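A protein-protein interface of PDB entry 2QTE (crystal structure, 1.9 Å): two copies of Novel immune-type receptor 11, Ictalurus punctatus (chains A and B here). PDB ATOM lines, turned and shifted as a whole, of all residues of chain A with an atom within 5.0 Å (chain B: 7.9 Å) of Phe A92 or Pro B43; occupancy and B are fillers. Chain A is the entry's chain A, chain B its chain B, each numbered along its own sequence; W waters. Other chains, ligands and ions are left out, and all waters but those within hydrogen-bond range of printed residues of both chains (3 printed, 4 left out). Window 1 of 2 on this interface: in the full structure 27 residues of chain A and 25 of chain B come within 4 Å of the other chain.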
ATOM      1  N   LEU A   6     -19.218 -13.890  12.084  1.00  0.00           N
ATOM      2  CA  LEU A   6     -19.174 -14.128  13.485  1.00  0.00           C
ATOM      3  C   LEU A   6     -18.660 -15.535  13.721  1.00  0.00           C
ATOM      4  O   LEU A   6     -18.920 -16.446  12.943  1.00  0.00           O
ATOM      5  CB  LEU A   6     -20.585 -14.058  14.080  1.00  0.00           C
ATOM      6  CG  LEU A   6     -21.370 -12.767  13.967  1.00  0.00           C
ATOM      7  CD1 LEU A   6     -22.765 -13.050  14.566  1.00  0.00           C
ATOM      8  CD2 LEU A   6     -20.622 -11.668  14.730  1.00  0.00           C
ATOM      9  N   ALA A  33     -14.570  -1.314  22.490  1.00  0.00           N
ATOM     10  CA  ALA A  33     -15.593  -1.800  23.390  1.00  0.00           C
ATOM     11  C   ALA A  33     -16.256  -3.023  22.818  1.00  0.00           C
ATOM     12  O   ALA A  33     -16.240  -3.237  21.602  1.00  0.00           O
ATOM     13  CB  ALA A  33     -16.663  -0.693  23.609  1.00  0.00           C
ATOM     14  N   TRP A  34     -16.904  -3.805  23.681  1.00  0.00           N
ATOM     15  CA  TRP A  34     -17.670  -4.928  23.240  1.00  0.00           C
ATOM     16  C   TRP A  34     -19.114  -4.506  23.372  1.00  0.00           C
ATOM     17  O   TRP A  34     -19.479  -3.824  24.330  1.00  0.00           O
ATOM     18  CB  TRP A  34     -17.444  -6.132  24.177  1.00  0.00           C
ATOM     19  CG  TRP A  34     -16.274  -7.013  23.855  1.00  0.00           C
ATOM     20  CD1 TRP A  34     -15.045  -6.981  24.421  1.00  0.00           C
ATOM     21  CD2 TRP A  34     -16.253  -8.090  22.895  1.00  0.00           C
ATOM     22  NE1 TRP A  34     -14.237  -7.963  23.860  1.00  0.00           N
ATOM     23  CE2 TRP A  34     -14.961  -8.646  22.920  1.00  0.00           C
ATOM     24  CE3 TRP A  34     -17.196  -8.620  22.016  1.00  0.00           C
ATOM     25  CZ2 TRP A  34     -14.606  -9.725  22.134  1.00  0.00           C
ATOM     26  CZ3 TRP A  34     -16.840  -9.680  21.208  1.00  0.00           C
ATOM     27  CH2 TRP A  34     -15.547 -10.206  21.254  1.00  0.00           C
ATOM     28  N   TYR A  35     -19.935  -4.854  22.391  1.00  0.00           N
ATOM     29  CA  TYR A  35     -21.355  -4.533  22.475  1.00  0.00           C
ATOM     30  C   TYR A  35     -22.028  -5.861  22.580  1.00  0.00           C
ATOM     31  O   TYR A  35     -21.527  -6.811  22.049  1.00  0.00           O
ATOM     32  CB  TYR A  35     -21.823  -3.808  21.209  1.00  0.00           C
ATOM     33  CG  TYR A  35     -21.315  -2.414  21.201  1.00  0.00           C
ATOM     34  CD1 TYR A  35     -19.944  -2.154  21.038  1.00  0.00           C
ATOM     35  CD2 TYR A  35     -22.166  -1.356  21.415  1.00  0.00           C
ATOM     36  CE1 TYR A  35     -19.465  -0.865  21.073  1.00  0.00           C
ATOM     37  CE2 TYR A  35     -21.691  -0.061  21.473  1.00  0.00           C
ATOM     38  CZ  TYR A  35     -20.339   0.156  21.296  1.00  0.00           C
ATOM     39  OH  TYR A  35     -19.887   1.424  21.348  1.00  0.00           O
ATOM     40  N   GLN A  37     -25.833  -7.973  22.125  1.00  0.00           N
ATOM     41  CA  GLN A  37     -27.209  -7.929  21.669  1.00  0.00           C
ATOM     42  C   GLN A  37     -27.873  -9.210  22.111  1.00  0.00           C
ATOM     43  O   GLN A  37     -27.506 -10.274  21.623  1.00  0.00           O
ATOM     44  CB  GLN A  37     -27.286  -7.886  20.132  1.00  0.00           C
ATOM     45  CG  GLN A  37     -28.719  -7.644  19.619  1.00  0.00           C
ATOM     46  CD  GLN A  37     -28.927  -8.096  18.208  1.00  0.00           C
ATOM     47  OE1 GLN A  37     -27.999  -8.591  17.578  1.00  0.00           O
ATOM     48  NE2 GLN A  37     -30.161  -7.948  17.704  1.00  0.00           N
ATOM     49  N   PRO A  43     -28.706  -3.791  20.092  1.00  0.00           N
ATOM     50  CA  PRO A  43     -27.443  -3.958  20.818  1.00  0.00           C
ATOM     51  C   PRO A  43     -27.073  -2.806  21.757  1.00  0.00           C
ATOM     52  O   PRO A  43     -27.451  -1.669  21.515  1.00  0.00           O
ATOM     53  CB  PRO A  43     -26.361  -3.964  19.703  1.00  0.00           C
ATOM     54  CG  PRO A  43     -27.096  -4.099  18.458  1.00  0.00           C
ATOM     55  CD  PRO A  43     -28.441  -3.540  18.678  1.00  0.00           C
ATOM     56  N   GLU A  90     -25.427 -12.170  20.854  1.00  0.00           N
ATOM     57  CA  GLU A  90     -24.284 -11.856  19.982  1.00  0.00           C
ATOM     58  C   GLU A  90     -23.468 -10.759  20.636  1.00  0.00           C
ATOM     59  O   GLU A  90     -24.026  -9.867  21.283  1.00  0.00           O
ATOM     60  CB  GLU A  90     -24.727 -11.516  18.545  1.00  0.00           C
ATOM     61  CG  GLU A  90     -25.707 -12.547  17.946  1.00  0.00           C
ATOM     62  CD  GLU A  90     -26.076 -12.348  16.497  1.00  0.00           C
ATOM     63  OE1 GLU A  90     -26.439 -11.210  16.085  1.00  0.00           O
ATOM     64  OE2 GLU A  90     -26.048 -13.355  15.762  1.00  0.00           O
ATOM     65  N   TYR A  91     -22.143 -10.850  20.471  1.00  0.00           N
ATOM     66  CA  TYR A  91     -21.223  -9.938  21.074  1.00  0.00           C
ATOM     67  C   TYR A  91     -20.297  -9.487  19.961  1.00  0.00           C
ATOM     68  O   TYR A  91     -19.644 -10.320  19.303  1.00  0.00           O
ATOM     69  CB  TYR A  91     -20.390 -10.621  22.186  1.00  0.00           C
ATOM     70  CG  TYR A  91     -21.214 -11.117  23.381  1.00  0.00           C
ATOM     71  CD1 TYR A  91     -22.007 -12.282  23.290  1.00  0.00           C
ATOM     72  CD2 TYR A  91     -21.169 -10.445  24.603  1.00  0.00           C
ATOM     73  CE1 TYR A  91     -22.783 -12.739  24.412  1.00  0.00           C
ATOM     74  CE2 TYR A  91     -21.901 -10.921  25.739  1.00  0.00           C
ATOM     75  CZ  TYR A  91     -22.692 -12.049  25.628  1.00  0.00           C
ATOM     76  OH  TYR A  91     -23.403 -12.481  26.751  1.00  0.00           O
ATOM     77  N   PHE A  92     -20.235  -8.178  19.793  1.00  0.00           N
ATOM     78  CA  PHE A  92     -19.503  -7.556  18.696  1.00  0.00           C
ATOM     79  C   PHE A  92     -18.412  -6.682  19.311  1.00  0.00           C
ATOM     80  O   PHE A  92     -18.680  -5.910  20.221  1.00  0.00           O
ATOM     81  CB  PHE A  92     -20.432  -6.622  17.885  1.00  0.00           C
ATOM     82  CG  PHE A  92     -21.764  -7.208  17.527  1.00  0.00           C
ATOM     83  CD1 PHE A  92     -21.847  -8.372  16.735  1.00  0.00           C
ATOM     84  CD2 PHE A  92     -22.939  -6.609  17.981  1.00  0.00           C
ATOM     85  CE1 PHE A  92     -23.061  -8.920  16.372  1.00  0.00           C
ATOM     86  CE2 PHE A  92     -24.231  -7.186  17.664  1.00  0.00           C
ATOM     87  CZ  PHE A  92     -24.292  -8.324  16.833  1.00  0.00           C
ATOM     88  N   CYS A  93     -17.196  -6.783  18.796  1.00  0.00           N
ATOM     89  CA  CYS A  93     -16.103  -5.962  19.234  1.00  0.00           C
ATOM     90  C   CYS A  93     -15.923  -4.890  18.188  1.00  0.00           C
ATOM     91  O   CYS A  93     -15.811  -5.177  17.029  1.00  0.00           O
ATOM     92  CB  CYS A  93     -14.840  -6.803  19.358  1.00  0.00           C
ATOM     93  SG  CYS A  93     -13.499  -5.961  20.135  1.00  0.00           S
ATOM     94  N   GLY A  94     -15.914  -3.651  18.604  1.00  0.00           N
ATOM     95  CA  GLY A  94     -15.784  -2.557  17.684  1.00  0.00           C
ATOM     96  C   GLY A  94     -15.098  -1.344  18.230  1.00  0.00           C
ATOM     97  O   GLY A  94     -14.974  -1.136  19.447  1.00  0.00           O
ATOM     98  N   PHE A 103     -16.944  -2.697  13.549  1.00  0.00           N
ATOM     99  CA  PHE A 103     -16.823  -3.936  14.341  1.00  0.00           C
ATOM    100  C   PHE A 103     -15.899  -4.872  13.631  1.00  0.00           C
ATOM    101  O   PHE A 103     -16.119  -5.168  12.465  1.00  0.00           O
ATOM    102  CB  PHE A 103     -18.194  -4.605  14.489  1.00  0.00           C
ATOM    103  CG  PHE A 103     -19.196  -3.780  15.254  1.00  0.00           C
ATOM    104  CD1 PHE A 103     -19.111  -3.676  16.641  1.00  0.00           C
ATOM    105  CD2 PHE A 103     -20.212  -3.087  14.602  1.00  0.00           C
ATOM    106  CE1 PHE A 103     -20.020  -2.916  17.346  1.00  0.00           C
ATOM    107  CE2 PHE A 103     -21.141  -2.349  15.311  1.00  0.00           C
ATOM    108  CZ  PHE A 103     -21.033  -2.242  16.676  1.00  0.00           C
ATOM    109  N   SER A 105     -14.771  -8.036  14.912  1.00  0.00           N
ATOM    110  CA  SER A 105     -15.044  -9.450  15.196  1.00  0.00           C
ATOM    111  C   SER A 105     -16.318  -9.598  16.031  1.00  0.00           C
ATOM    112  O   SER A 105     -16.854  -8.618  16.563  1.00  0.00           O
ATOM    113  CB  SER A 105     -13.845 -10.138  15.858  1.00  0.00           C
ATOM    114  OG  SER A 105     -13.388  -9.455  17.023  1.00  0.00           O
ATOM    115  N   GLY A 106     -16.833 -10.807  16.118  1.00  0.00           N
ATOM    116  CA  GLY A 106     -17.952 -11.038  17.033  1.00  0.00           C
ATOM    117  C   GLY A 106     -18.225 -12.503  17.189  1.00  0.00           C
ATOM    118  O   GLY A 106     -17.707 -13.318  16.431  1.00  0.00           O
ATOM    119  N   TYR B  35     -27.125   0.869  10.877  1.00  0.00           N
ATOM    120  CA  TYR B  35     -26.131  -0.227  10.761  1.00  0.00           C
ATOM    121  C   TYR B  35     -26.846  -1.434  10.269  1.00  0.00           C
ATOM    122  O   TYR B  35     -28.016  -1.631  10.606  1.00  0.00           O
ATOM    123  CB  TYR B  35     -25.476  -0.491  12.114  1.00  0.00           C
ATOM    124  CG  TYR B  35     -24.498   0.612  12.443  1.00  0.00           C
ATOM    125  CD1 TYR B  35     -24.948   1.926  12.746  1.00  0.00           C
ATOM    126  CD2 TYR B  35     -23.121   0.365  12.393  1.00  0.00           C
ATOM    127  CE1 TYR B  35     -24.038   2.943  13.028  1.00  0.00           C
ATOM    128  CE2 TYR B  35     -22.207   1.371  12.660  1.00  0.00           C
ATOM    129  CZ  TYR B  35     -22.672   2.649  12.958  1.00  0.00           C
ATOM    130  OH  TYR B  35     -21.758   3.612  13.210  1.00  0.00           O
ATOM    131  N   ARG B  36     -26.193  -2.207   9.399  1.00  0.00           N
ATOM    132  CA  ARG B  36     -26.864  -3.330   8.846  1.00  0.00           C
ATOM    133  C   ARG B  36     -26.197  -4.624   9.237  1.00  0.00           C
ATOM    134  O   ARG B  36     -24.986  -4.752   9.096  1.00  0.00           O
ATOM    135  CB  ARG B  36     -26.932  -3.225   7.321  1.00  0.00           C
ATOM    136  CG  ARG B  36     -27.574  -4.392   6.650  1.00  0.00           C
ATOM    137  CD  ARG B  36     -27.538  -4.169   5.175  1.00  0.00           C
ATOM    138  NE  ARG B  36     -28.057  -5.295   4.445  1.00  0.00           N
ATOM    139  CZ  ARG B  36     -28.303  -5.307   3.138  1.00  0.00           C
ATOM    140  NH1 ARG B  36     -28.077  -4.223   2.403  1.00  0.00           N
ATOM    141  NH2 ARG B  36     -28.763  -6.421   2.575  1.00  0.00           N
ATOM    142  N   GLN B  37     -26.998  -5.586   9.695  1.00  0.00           N
ATOM    143  CA  GLN B  37     -26.446  -6.904  10.053  1.00  0.00           C
ATOM    144  C   GLN B  37     -27.099  -8.065   9.315  1.00  0.00           C
ATOM    145  O   GLN B  37     -28.254  -8.439   9.605  1.00  0.00           O
ATOM    146  CB  GLN B  37     -26.470  -7.155  11.577  1.00  0.00           C
ATOM    147  CG  GLN B  37     -25.796  -8.509  11.907  1.00  0.00           C
ATOM    148  CD  GLN B  37     -25.968  -9.052  13.349  1.00  0.00           C
ATOM    149  OE1 GLN B  37     -26.944  -8.745  14.071  1.00  0.00           O
ATOM    150  NE2 GLN B  37     -25.054  -9.974  13.718  1.00  0.00           N
ATOM    151  N   SER B  38     -26.343  -8.664   8.395  1.00  0.00           N
ATOM    152  CA  SER B  38     -26.707  -9.946   7.755  1.00  0.00           C
ATOM    153  C   SER B  38     -26.522 -11.125   8.738  1.00  0.00           C
ATOM    154  O   SER B  38     -25.685 -11.053   9.622  1.00  0.00           O
ATOM    155  CB  SER B  38     -25.912 -10.147   6.436  1.00  0.00           C
ATOM    156  OG  SER B  38     -26.338  -9.193   5.483  1.00  0.00           O
ATOM    157  N   GLY B  40     -25.231 -13.938  10.820  1.00  0.00           N
ATOM    158  CA  GLY B  40     -23.889 -14.546  11.014  1.00  0.00           C
ATOM    159  C   GLY B  40     -22.731 -13.640  10.672  1.00  0.00           C
ATOM    160  O   GLY B  40     -21.591 -14.111  10.624  1.00  0.00           O
ATOM    161  N   LYS B  41     -23.029 -12.368  10.353  1.00  0.00           N
ATOM    162  CA  LYS B  41     -22.035 -11.314  10.079  1.00  0.00           C
ATOM    163  C   LYS B  41     -21.947 -10.265  11.178  1.00  0.00           C
ATOM    164  O   LYS B  41     -22.839 -10.146  12.046  1.00  0.00           O
ATOM    165  CB  LYS B  41     -22.279 -10.611   8.711  1.00  0.00           C
ATOM    166  CG  LYS B  41     -22.436 -11.522   7.532  1.00  0.00           C
ATOM    167  CD  LYS B  41     -21.111 -12.227   7.331  1.00  0.00           C
ATOM    168  CE  LYS B  41     -21.047 -13.071   6.032  1.00  0.00           C
ATOM    169  NZ  LYS B  41     -22.217 -13.987   5.865  1.00  0.00           N
ATOM    170  N   VAL B  42     -20.812  -9.564  11.237  1.00  0.00           N
ATOM    171  CA  VAL B  42     -20.720  -8.415  12.151  1.00  0.00           C
ATOM    172  C   VAL B  42     -21.632  -7.323  11.563  1.00  0.00           C
ATOM    173  O   VAL B  42     -21.852  -7.323  10.354  1.00  0.00           O
ATOM    174  CB  VAL B  42     -19.263  -7.881  12.327  1.00  0.00           C
ATOM    175  CG1 VAL B  42     -18.358  -8.969  12.987  1.00  0.00           C
ATOM    176  CG2 VAL B  42     -18.685  -7.412  11.010  1.00  0.00           C
ATOM    177  N   PRO B  43     -22.228  -6.434  12.401  1.00  0.00           N
ATOM    178  CA  PRO B  43     -22.926  -5.285  11.825  1.00  0.00           C
ATOM    179  C   PRO B  43     -21.951  -4.362  11.104  1.00  0.00           C
ATOM    180  O   PRO B  43     -20.766  -4.346  11.448  1.00  0.00           O
ATOM    181  CB  PRO B  43     -23.557  -4.590  13.048  1.00  0.00           C
ATOM    182  CG  PRO B  43     -23.684  -5.778  14.087  1.00  0.00           C
ATOM    183  CD  PRO B  43     -22.356  -6.455  13.868  1.00  0.00           C
ATOM    184  N   GLN B  44     -22.479  -3.601  10.133  1.00  0.00           N
ATOM    185  CA  GLN B  44     -21.710  -2.641   9.348  1.00  0.00           C
ATOM    186  C   GLN B  44     -22.499  -1.356   9.203  1.00  0.00           C
ATOM    187  O   GLN B  44     -23.713  -1.375   8.952  1.00  0.00           O
ATOM    188  CB  GLN B  44     -21.446  -3.195   7.946  1.00  0.00           C
ATOM    189  CG  GLN B  44     -20.595  -4.469   7.909  1.00  0.00           C
ATOM    190  CD  GLN B  44     -19.846  -4.609   6.582  1.00  0.00           C
ATOM    191  OE1 GLN B  44     -18.607  -4.659   6.542  1.00  0.00           O
ATOM    192  NE2 GLN B  44     -20.588  -4.669   5.497  1.00  0.00           N
ATOM    193  N   TYR B  45     -21.787  -0.241   9.364  1.00  0.00           N
ATOM    194  CA  TYR B  45     -22.334   1.086   9.082  1.00  0.00           C
ATOM    195  C   TYR B  45     -22.918   1.056   7.698  1.00  0.00           C
ATOM    196  O   TYR B  45     -22.277   0.566   6.756  1.00  0.00           O
ATOM    197  CB  TYR B  45     -21.213   2.133   9.154  1.00  0.00           C
ATOM    198  CG  TYR B  45     -21.366   3.314   8.241  1.00  0.00           C
ATOM    199  CD1 TYR B  45     -22.519   4.102   8.286  1.00  0.00           C
ATOM    200  CD2 TYR B  45     -20.356   3.679   7.356  1.00  0.00           C
ATOM    201  CE1 TYR B  45     -22.688   5.191   7.453  1.00  0.00           C
ATOM    202  CE2 TYR B  45     -20.510   4.809   6.496  1.00  0.00           C
ATOM    203  CZ  TYR B  45     -21.693   5.555   6.580  1.00  0.00           C
ATOM    204  OH  TYR B  45     -21.922   6.671   5.787  1.00  0.00           O
ATOM    205  N   PHE B  46     -24.115   1.623   7.543  1.00  0.00           N
ATOM    206  CA  PHE B  46     -24.790   1.471   6.288  1.00  0.00           C
ATOM    207  C   PHE B  46     -25.125   2.781   5.534  1.00  0.00           C
ATOM    208  O   PHE B  46     -25.011   2.875   4.305  1.00  0.00           O
ATOM    209  CB  PHE B  46     -26.014   0.601   6.599  1.00  0.00           C
ATOM    210  CG  PHE B  46     -26.780   0.207   5.437  1.00  0.00           C
ATOM    211  CD1 PHE B  46     -26.146  -0.336   4.322  1.00  0.00           C
ATOM    212  CD2 PHE B  46     -28.180   0.296   5.460  1.00  0.00           C
ATOM    213  CE1 PHE B  46     -26.867  -0.735   3.221  1.00  0.00           C
ATOM    214  CE2 PHE B  46     -28.923  -0.106   4.361  1.00  0.00           C
ATOM    215  CZ  PHE B  46     -28.296  -0.612   3.229  1.00  0.00           C
ATOM    216  N   GLU B  90     -30.863  -7.677  10.378  1.00  0.00           N
ATOM    217  CA  GLU B  90     -31.205  -6.746  11.420  1.00  0.00           C
ATOM    218  C   GLU B  90     -30.649  -5.384  11.144  1.00  0.00           C
ATOM    219  O   GLU B  90     -29.465  -5.236  10.682  1.00  0.00           O
ATOM    220  CB  GLU B  90     -30.752  -7.300  12.778  1.00  0.00           C
ATOM    221  CG  GLU B  90     -31.590  -8.599  13.046  1.00  0.00           C
ATOM    222  CD  GLU B  90     -31.381  -9.172  14.442  1.00  0.00           C
ATOM    223  OE1 GLU B  90     -30.317  -8.962  15.042  1.00  0.00           O
ATOM    224  OE2 GLU B  90     -32.278  -9.871  14.923  1.00  0.00           O
ATOM    225  N   PHE B  92     -30.096  -1.451  12.647  1.00  0.00           N
ATOM    226  CA  PHE B  92     -30.008  -0.684  13.896  1.00  0.00           C
ATOM    227  C   PHE B  92     -29.704   0.765  13.655  1.00  0.00           C
ATOM    228  O   PHE B  92     -28.786   1.107  12.895  1.00  0.00           O
ATOM    229  CB  PHE B  92     -28.916  -1.224  14.861  1.00  0.00           C
ATOM    230  CG  PHE B  92     -28.855  -2.724  14.958  1.00  0.00           C
ATOM    231  CD1 PHE B  92     -29.921  -3.455  15.461  1.00  0.00           C
ATOM    232  CD2 PHE B  92     -27.695  -3.408  14.623  1.00  0.00           C
ATOM    233  CE1 PHE B  92     -29.836  -4.878  15.548  1.00  0.00           C
ATOM    234  CE2 PHE B  92     -27.601  -4.815  14.747  1.00  0.00           C
ATOM    235  CZ  PHE B  92     -28.663  -5.526  15.166  1.00  0.00           C
ATOM    236  N   PHE B 103     -27.746   2.780  20.348  1.00  0.00           N
ATOM    237  CA  PHE B 103     -28.784   2.422  19.381  1.00  0.00           C
ATOM    238  C   PHE B 103     -30.166   2.746  19.966  1.00  0.00           C
ATOM    239  O   PHE B 103     -30.390   2.461  21.102  1.00  0.00           O
ATOM    240  CB  PHE B 103     -28.641   0.954  19.013  1.00  0.00           C
ATOM    241  CG  PHE B 103     -27.342   0.650  18.300  1.00  0.00           C
ATOM    242  CD1 PHE B 103     -27.162   1.063  17.005  1.00  0.00           C
ATOM    243  CD2 PHE B 103     -26.339  -0.070  18.909  1.00  0.00           C
ATOM    244  CE1 PHE B 103     -25.998   0.820  16.323  1.00  0.00           C
ATOM    245  CE2 PHE B 103     -25.146  -0.339  18.219  1.00  0.00           C
ATOM    246  CZ  PHE B 103     -24.983   0.113  16.924  1.00  0.00           C
HETATM  247  O   HOH W   1     -21.464 -17.175  11.629  1.00  0.00           O
HETATM  248  O   HOH W   2     -18.452  -2.907  10.941  1.00  0.00           O
HETATM  249  O   HOH W   3     -26.494 -13.426  13.206  1.00  0.00           O
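Printed residues of chain B that touch a printed residue of chain A: Gln B37, Gly B40, Lys B41, Val B42, Pro B43, Glu B90, Phe B92 and Phe B103.
Hydrophobic or aromatic side chains of chain B that line the printed part of chain A: Val B42, Pro B43, Phe B92 and Phe B103.
Among the printed residues, 16 pairs touch across the chains.
Among the printed residues, no Asp or Glu carboxylate lies within 4 Å of a Lys or Arg side-chain nitrogen of the other chain.
The backbone NH of Cys A93 sits at hydrogen-bond distance from the backbone carbonyl oxygen of Ser A105, 2.9 Å away.
The backbone carbonyl oxygen (O) of Glu B90 lies within hydrogen-bond range of the backbone NH (N) of Gln B37, 2.7 Å away.
The side-chain amide nitrogen of Gln B37 lies within hydrogen-bond range of the backbone carbonyl oxygen of Lys B41, 2.8 Å away.
N of Tyr B35 is in hydrogen-bond range of O of Phe B92 (2.6 Å).
N of Tyr A35 is in hydrogen-bond range of O of Phe A92, 2.7 Å away.
The backbone carbonyl oxygen (O) of Glu A90 sits at hydrogen-bond distance from the backbone NH (N) of Gln A37.
Gln B37 touches its own counterpart, Gln A37.
Gln A37 touches Glu B90, and with the chains exchanged Glu A90 touches Gln B37.
Pro A43 touches Phe B92, and with the chains exchanged Phe A92 touches Pro B43.
Pro A43 touches Phe B103, and with the chains exchanged Phe A103 touches Pro B43.
6 positions are printed for both chains.
Of the 16 pairs that touch across the chains among the printed residues, 9 have their exchanged pair printed and touching as well.
Among the printed residues, pairs that only touch across the chains: Pro A43 with Phe B103 (3.3 Å), Phe A103 with Pro B43 (3.4 Å), Phe A92 with Gln B37 (3.5 Å), Phe A92 with Pro B43 (3.5 Å), Pro A43 with Phe B92 (3.5 Å), Leu A6 with Lys B41 (3.6 Å), Gln A37 with Gln B37 (3.7 Å), Phe A103 with Val B42 (3.7 Å), Ser A105 with Val B42 (3.7 Å), Gln A37 with Phe B92 (3.8 Å), Leu A6 with Gln B37 (3.9 Å), Leu A6 with Val B42 (3.9 Å) and Gly A106 with Val B42 (3.9 Å).
Water W3 lies within hydrogen-bond range of OE2 of Glu A90 (2.6 Å) and N of Gly B40 (2.7 Å).
Water W2 lies within hydrogen-bond range of O of Pro B43 (2.8 Å) and N of Phe A103 (3.0 Å).
Water W1 lies within hydrogen-bond range of the backbone carbonyl oxygen of Leu A6 (3.0 Å) and the backbone carbonyl oxygen of Gly B40 (3.2 Å).
Phe A92 touches two residues of chain B.
Pro B43 touches just these residues of chain A: Phe A92 and Phe A103.
Printed residues of chain A within 4 Å of Phe B103: Pro A43.
Of the printed residues of chain A, Val B42 touches Leu A6, Phe A103, Ser A105 and Gly A106.
Printed residues of chain B within 4 Å of Gln A37: Gln B37 (3.7 Å), Glu B90 (2.9 Å) and Phe B92 (3.8 Å).
Of the printed residues of chain B, Gly A106 touches Val B42.
Of the printed residues of chain A, Gly B40 touches Leu A6 (2.8 Å).
The nearest residue of chain B that does not touch Phe A92 is Lys B41 (4.5 Å).
The side-chain amide nitrogen of Gln B37 lies within hydrogen-bond range of the side-chain carboxylate of Glu A90.
The side-chain carboxylate (OE1) of Glu B90 lies within hydrogen-bond range of the side-chain amide nitrogen (NE2) of Gln A37 (2.9 Å).
The backbone NH (N) of Leu A6 lies within hydrogen-bond range of the backbone carbonyl oxygen (O) of Gly B40, 2.8 Å away.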
